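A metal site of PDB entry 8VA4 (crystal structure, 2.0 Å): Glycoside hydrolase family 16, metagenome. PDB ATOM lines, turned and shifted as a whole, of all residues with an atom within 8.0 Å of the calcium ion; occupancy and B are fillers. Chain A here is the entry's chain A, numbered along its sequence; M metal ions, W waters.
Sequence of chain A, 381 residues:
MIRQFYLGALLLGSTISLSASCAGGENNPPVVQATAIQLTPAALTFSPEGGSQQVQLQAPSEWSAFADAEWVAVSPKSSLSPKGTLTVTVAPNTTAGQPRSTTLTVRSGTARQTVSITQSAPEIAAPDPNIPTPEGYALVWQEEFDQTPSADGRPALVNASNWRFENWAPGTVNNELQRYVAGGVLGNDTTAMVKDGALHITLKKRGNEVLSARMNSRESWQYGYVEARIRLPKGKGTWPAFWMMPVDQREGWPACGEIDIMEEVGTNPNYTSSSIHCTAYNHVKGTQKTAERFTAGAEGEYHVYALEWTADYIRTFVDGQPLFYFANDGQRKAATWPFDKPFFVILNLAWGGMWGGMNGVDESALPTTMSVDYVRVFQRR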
ATOM      1  N   GLU A 143     -29.296 -23.938 -15.489  1.00  0.00           N
ATOM      2  CA  GLU A 143     -28.604 -23.741 -14.221  1.00  0.00           C
ATOM      3  C   GLU A 143     -27.634 -22.590 -14.438  1.00  0.00           C
ATOM      4  O   GLU A 143     -26.543 -22.776 -14.980  1.00  0.00           O
ATOM      5  CB  GLU A 143     -27.896 -25.016 -13.768  1.00  0.00           C
ATOM      6  CG  GLU A 143     -26.939 -24.834 -12.602  1.00  0.00           C
ATOM      7  CD  GLU A 143     -27.624 -24.356 -11.327  1.00  0.00           C
ATOM      8  OE1 GLU A 143     -27.934 -23.154 -11.231  1.00  0.00           O
ATOM      9  OE2 GLU A 143     -27.839 -25.179 -10.416  1.00  0.00           O
ATOM     10  N   GLU A 144     -28.042 -21.392 -14.035  1.00  0.00           N
ATOM     11  CA  GLU A 144     -27.227 -20.192 -14.198  1.00  0.00           C
ATOM     12  C   GLU A 144     -26.246 -20.002 -13.058  1.00  0.00           C
ATOM     13  O   GLU A 144     -25.451 -19.057 -13.087  1.00  0.00           O
ATOM     14  CB  GLU A 144     -28.108 -18.956 -14.319  1.00  0.00           C
ATOM     15  CG  GLU A 144     -29.051 -18.975 -15.511  1.00  0.00           C
ATOM     16  CD  GLU A 144     -28.302 -19.006 -16.819  1.00  0.00           C
ATOM     17  OE1 GLU A 144     -27.427 -18.139 -17.032  1.00  0.00           O
ATOM     18  OE2 GLU A 144     -28.588 -19.906 -17.650  1.00  0.00           O
ATOM     19  N   PHE A 145     -26.292 -20.874 -12.045  1.00  0.00           N
ATOM     20  CA  PHE A 145     -25.436 -20.780 -10.859  1.00  0.00           C
ATOM     21  C   PHE A 145     -25.488 -19.367 -10.269  1.00  0.00           C
ATOM     22  O   PHE A 145     -24.465 -18.749  -9.973  1.00  0.00           O
ATOM     23  CB  PHE A 145     -24.007 -21.200 -11.178  1.00  0.00           C
ATOM     24  CG  PHE A 145     -23.875 -22.671 -11.511  1.00  0.00           C
ATOM     25  CD1 PHE A 145     -24.141 -23.640 -10.565  1.00  0.00           C
ATOM     26  CD2 PHE A 145     -23.461 -23.073 -12.780  1.00  0.00           C
ATOM     27  CE1 PHE A 145     -24.003 -24.995 -10.867  1.00  0.00           C
ATOM     28  CE2 PHE A 145     -23.329 -24.427 -13.095  1.00  0.00           C
ATOM     29  CZ  PHE A 145     -23.604 -25.379 -12.129  1.00  0.00           C
ATOM     30  N   ASP A 146     -26.706 -18.861 -10.096  1.00  0.00           N
ATOM     31  CA  ASP A 146     -26.936 -17.517  -9.568  1.00  0.00           C
ATOM     32  C   ASP A 146     -26.367 -17.352  -8.160  1.00  0.00           C
ATOM     33  O   ASP A 146     -27.110 -17.322  -7.188  1.00  0.00           O
ATOM     34  CB  ASP A 146     -28.433 -17.220  -9.562  1.00  0.00           C
ATOM     35  CG  ASP A 146     -29.050 -17.302 -10.946  1.00  0.00           C
ATOM     36  OD1 ASP A 146     -28.416 -16.840 -11.912  1.00  0.00           O
ATOM     37  OD2 ASP A 146     -30.171 -17.846 -11.073  1.00  0.00           O
ATOM     38  N   VAL A 194     -20.680 -22.015  -5.175  1.00  0.00           N
ATOM     39  CA  VAL A 194     -21.033 -21.028  -6.187  1.00  0.00           C
ATOM     40  C   VAL A 194     -20.522 -19.663  -5.739  1.00  0.00           C
ATOM     41  O   VAL A 194     -20.768 -19.252  -4.599  1.00  0.00           O
ATOM     42  CB  VAL A 194     -22.558 -20.987  -6.438  1.00  0.00           C
ATOM     43  CG1 VAL A 194     -22.895 -19.901  -7.439  1.00  0.00           C
ATOM     44  CG2 VAL A 194     -23.028 -22.335  -6.950  1.00  0.00           C
ATOM     45  N   LYS A 195     -19.802 -18.989  -6.623  1.00  0.00           N
ATOM     46  CA  LYS A 195     -19.243 -17.679  -6.314  1.00  0.00           C
ATOM     47  C   LYS A 195     -19.210 -16.865  -7.601  1.00  0.00           C
ATOM     48  O   LYS A 195     -18.808 -17.373  -8.643  1.00  0.00           O
ATOM     49  CB  LYS A 195     -17.837 -17.826  -5.726  1.00  0.00           C
ATOM     50  CG  LYS A 195     -17.166 -16.519  -5.343  1.00  0.00           C
ATOM     51  CD  LYS A 195     -15.767 -16.782  -4.786  1.00  0.00           C
ATOM     52  CE  LYS A 195     -14.996 -15.491  -4.571  1.00  0.00           C
ATOM     53  NZ  LYS A 195     -14.757 -14.769  -5.852  1.00  0.00           N
ATOM     54  N   ASP A 196     -19.667 -15.613  -7.508  1.00  0.00           N
ATOM     55  CA  ASP A 196     -19.667 -14.674  -8.631  1.00  0.00           C
ATOM     56  C   ASP A 196     -20.470 -15.206  -9.827  1.00  0.00           C
ATOM     57  O   ASP A 196     -20.117 -14.960 -10.984  1.00  0.00           O
ATOM     58  CB  ASP A 196     -18.242 -14.335  -9.070  1.00  0.00           C
ATOM     59  CG  ASP A 196     -17.415 -13.755  -7.945  1.00  0.00           C
ATOM     60  OD1 ASP A 196     -17.917 -12.866  -7.245  1.00  0.00           O
ATOM     61  OD2 ASP A 196     -16.264 -14.209  -7.747  1.00  0.00           O
ATOM     62  N   GLY A 197     -21.541 -15.936  -9.548  1.00  0.00           N
ATOM     63  CA  GLY A 197     -22.406 -16.417 -10.607  1.00  0.00           C
ATOM     64  C   GLY A 197     -21.901 -17.641 -11.332  1.00  0.00           C
ATOM     65  O   GLY A 197     -22.373 -17.929 -12.437  1.00  0.00           O
ATOM     66  N   ALA A 198     -20.969 -18.387 -10.749  1.00  0.00           N
ATOM     67  CA  ALA A 198     -20.409 -19.566 -11.397  1.00  0.00           C
ATOM     68  C   ALA A 198     -20.172 -20.675 -10.383  1.00  0.00           C
ATOM     69  O   ALA A 198     -19.798 -20.408  -9.235  1.00  0.00           O
ATOM     70  CB  ALA A 198     -19.093 -19.245 -12.120  1.00  0.00           C
ATOM     71  N   LEU A 199     -20.408 -21.905 -10.810  1.00  0.00           N
ATOM     72  CA  LEU A 199     -19.966 -23.063 -10.036  1.00  0.00           C
ATOM     73  C   LEU A 199     -18.442 -23.126 -10.024  1.00  0.00           C
ATOM     74  O   LEU A 199     -17.790 -22.880 -11.043  1.00  0.00           O
ATOM     75  CB  LEU A 199     -20.543 -24.330 -10.630  1.00  0.00           C
ATOM     76  CG  LEU A 199     -19.872 -25.644 -10.239  1.00  0.00           C
ATOM     77  CD1 LEU A 199     -20.213 -26.004  -8.796  1.00  0.00           C
ATOM     78  CD2 LEU A 199     -20.293 -26.749 -11.192  1.00  0.00           C
ATOM     79  N   ARG A 229     -20.694 -23.197 -20.192  1.00  0.00           N
ATOM     80  CA  ARG A 229     -19.557 -22.280 -20.295  1.00  0.00           C
ATOM     81  C   ARG A 229     -18.589 -22.623 -19.162  1.00  0.00           C
ATOM     82  O   ARG A 229     -18.913 -22.433 -17.985  1.00  0.00           O
ATOM     83  CB  ARG A 229     -20.023 -20.825 -20.224  1.00  0.00           C
ATOM     84  CG  ARG A 229     -18.953 -19.826 -20.591  1.00  0.00           C
ATOM     85  CD  ARG A 229     -19.558 -18.461 -20.885  1.00  0.00           C
ATOM     86  NE  ARG A 229     -18.524 -17.451 -21.088  1.00  0.00           N
ATOM     87  CZ  ARG A 229     -18.106 -16.601 -20.163  1.00  0.00           C
ATOM     88  NH1 ARG A 229     -18.645 -16.582 -18.956  1.00  0.00           N
ATOM     89  NH2 ARG A 229     -17.137 -15.750 -20.456  1.00  0.00           N
ATOM     90  N   TYR A 302     -12.920 -18.932 -19.849  1.00  0.00           N
ATOM     91  CA  TYR A 302     -14.196 -19.558 -20.156  1.00  0.00           C
ATOM     92  C   TYR A 302     -14.323 -19.817 -21.653  1.00  0.00           C
ATOM     93  O   TYR A 302     -13.986 -18.969 -22.479  1.00  0.00           O
ATOM     94  CB  TYR A 302     -15.352 -18.677 -19.685  1.00  0.00           C
ATOM     95  CG  TYR A 302     -15.652 -18.745 -18.199  1.00  0.00           C
ATOM     96  CD1 TYR A 302     -16.330 -19.833 -17.661  1.00  0.00           C
ATOM     97  CD2 TYR A 302     -15.275 -17.725 -17.352  1.00  0.00           C
ATOM     98  CE1 TYR A 302     -16.624 -19.904 -16.310  1.00  0.00           C
ATOM     99  CE2 TYR A 302     -15.552 -17.785 -15.993  1.00  0.00           C
ATOM    100  CZ  TYR A 302     -16.223 -18.876 -15.489  1.00  0.00           C
ATOM    101  OH  TYR A 302     -16.501 -18.929 -14.136  1.00  0.00           O
ATOM    102  N   VAL A 372     -17.807 -23.311 -13.854  1.00  0.00           N
ATOM    103  CA  VAL A 372     -18.904 -23.444 -14.809  1.00  0.00           C
ATOM    104  C   VAL A 372     -19.815 -22.233 -14.632  1.00  0.00           C
ATOM    105  O   VAL A 372     -20.450 -22.068 -13.588  1.00  0.00           O
ATOM    106  CB  VAL A 372     -19.668 -24.754 -14.625  1.00  0.00           C
ATOM    107  CG1 VAL A 372     -20.689 -24.926 -15.740  1.00  0.00           C
ATOM    108  CG2 VAL A 372     -18.713 -25.924 -14.597  1.00  0.00           C
ATOM    109  N   ASP A 373     -19.876 -21.392 -15.669  1.00  0.00           N
ATOM    110  CA  ASP A 373     -20.747 -20.218 -15.610  1.00  0.00           C
ATOM    111  C   ASP A 373     -22.212 -20.611 -15.682  1.00  0.00           C
ATOM    112  O   ASP A 373     -23.054 -20.017 -14.992  1.00  0.00           O
ATOM    113  CB  ASP A 373     -20.366 -19.255 -16.747  1.00  0.00           C
ATOM    114  CG  ASP A 373     -21.167 -17.974 -16.710  1.00  0.00           C
ATOM    115  OD1 ASP A 373     -21.685 -17.599 -15.635  1.00  0.00           O
ATOM    116  OD2 ASP A 373     -21.270 -17.321 -17.770  1.00  0.00           O
ATOM    117  N   TYR A 374     -22.541 -21.603 -16.511  1.00  0.00           N
ATOM    118  CA  TYR A 374     -23.920 -22.039 -16.645  1.00  0.00           C
ATOM    119  C   TYR A 374     -23.958 -23.391 -17.341  1.00  0.00           C
ATOM    120  O   TYR A 374     -22.998 -23.791 -18.016  1.00  0.00           O
ATOM    121  CB  TYR A 374     -24.780 -21.014 -17.407  1.00  0.00           C
ATOM    122  CG  TYR A 374     -24.349 -20.759 -18.846  1.00  0.00           C
ATOM    123  CD1 TYR A 374     -24.661 -21.658 -19.859  1.00  0.00           C
ATOM    124  CD2 TYR A 374     -23.647 -19.613 -19.184  1.00  0.00           C
ATOM    125  CE1 TYR A 374     -24.277 -21.435 -21.161  1.00  0.00           C
ATOM    126  CE2 TYR A 374     -23.251 -19.378 -20.492  1.00  0.00           C
ATOM    127  CZ  TYR A 374     -23.567 -20.297 -21.480  1.00  0.00           C
ATOM    128  OH  TYR A 374     -23.197 -20.079 -22.784  1.00  0.00           O
ATOM    129  N   VAL A 375     -25.067 -24.098 -17.159  1.00  0.00           N
ATOM    130  CA  VAL A 375     -25.431 -25.262 -17.954  1.00  0.00           C
ATOM    131  C   VAL A 375     -26.845 -25.021 -18.458  1.00  0.00           C
ATOM    132  O   VAL A 375     -27.769 -24.821 -17.649  1.00  0.00           O
ATOM    133  CB  VAL A 375     -25.357 -26.568 -17.151  1.00  0.00           C
ATOM    134  CG1 VAL A 375     -25.632 -27.764 -18.056  1.00  0.00           C
ATOM    135  CG2 VAL A 375     -24.019 -26.717 -16.464  1.00  0.00           C
ATOM    136  N   ARG A 376     -27.018 -25.020 -19.767  1.00  0.00           N
ATOM    137  CA  ARG A 376     -28.323 -24.786 -20.374  1.00  0.00           C
ATOM    138  C   ARG A 376     -28.690 -25.962 -21.268  1.00  0.00           C
ATOM    139  O   ARG A 376     -27.828 -26.544 -21.919  1.00  0.00           O
ATOM    140  CB  ARG A 376     -28.330 -23.478 -21.175  1.00  0.00           C
ATOM    141  CG  ARG A 376     -28.161 -22.249 -20.300  1.00  0.00           C
ATOM    142  CD  ARG A 376     -27.872 -21.000 -21.111  1.00  0.00           C
ATOM    143  NE  ARG A 376     -27.551 -19.874 -20.244  1.00  0.00           N
ATOM    144  CZ  ARG A 376     -26.994 -18.740 -20.650  1.00  0.00           C
ATOM    145  NH1 ARG A 376     -26.715 -18.531 -21.930  1.00  0.00           N
ATOM    146  NH2 ARG A 376     -26.713 -17.791 -19.755  1.00  0.00           N
HETATM  147 CA    CA M   1     -23.726 -17.736 -14.176  1.00  0.00          CA
HETATM  148  O   HOH W   1     -25.377 -16.051 -12.948  1.00  0.00           O
HETATM  149  O   HOH W   2     -23.019 -15.468 -14.251  1.00  0.00           O
HETATM  150  O   HOH W   3     -25.072 -17.481 -16.158  1.00  0.00           O
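Three residues have an atom within 4 Å of the calcium ion: Glu 144, Gly 197 and Asp 373.
The nearest printed residue that does not touch the calcium ion is Phe 145 (4.4 Å).
The guanidinium group of Arg 229 is in salt-bridge range of the side-chain carboxylate of Asp 373 (3.0 Å).
OE2 of Glu 144 is in salt-bridge range of NE of Arg 376 (2.8 Å).
The calcium ion is bound by O of Gly 197 (2.2 Å), water W2 (2.4 Å), water W3 (2.4 Å), O of Glu 144 (2.4 Å), OD1 of Asp 373 (2.5 Å), O of Asp 373 (2.5 Å) and water W1 (2.7 Å).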
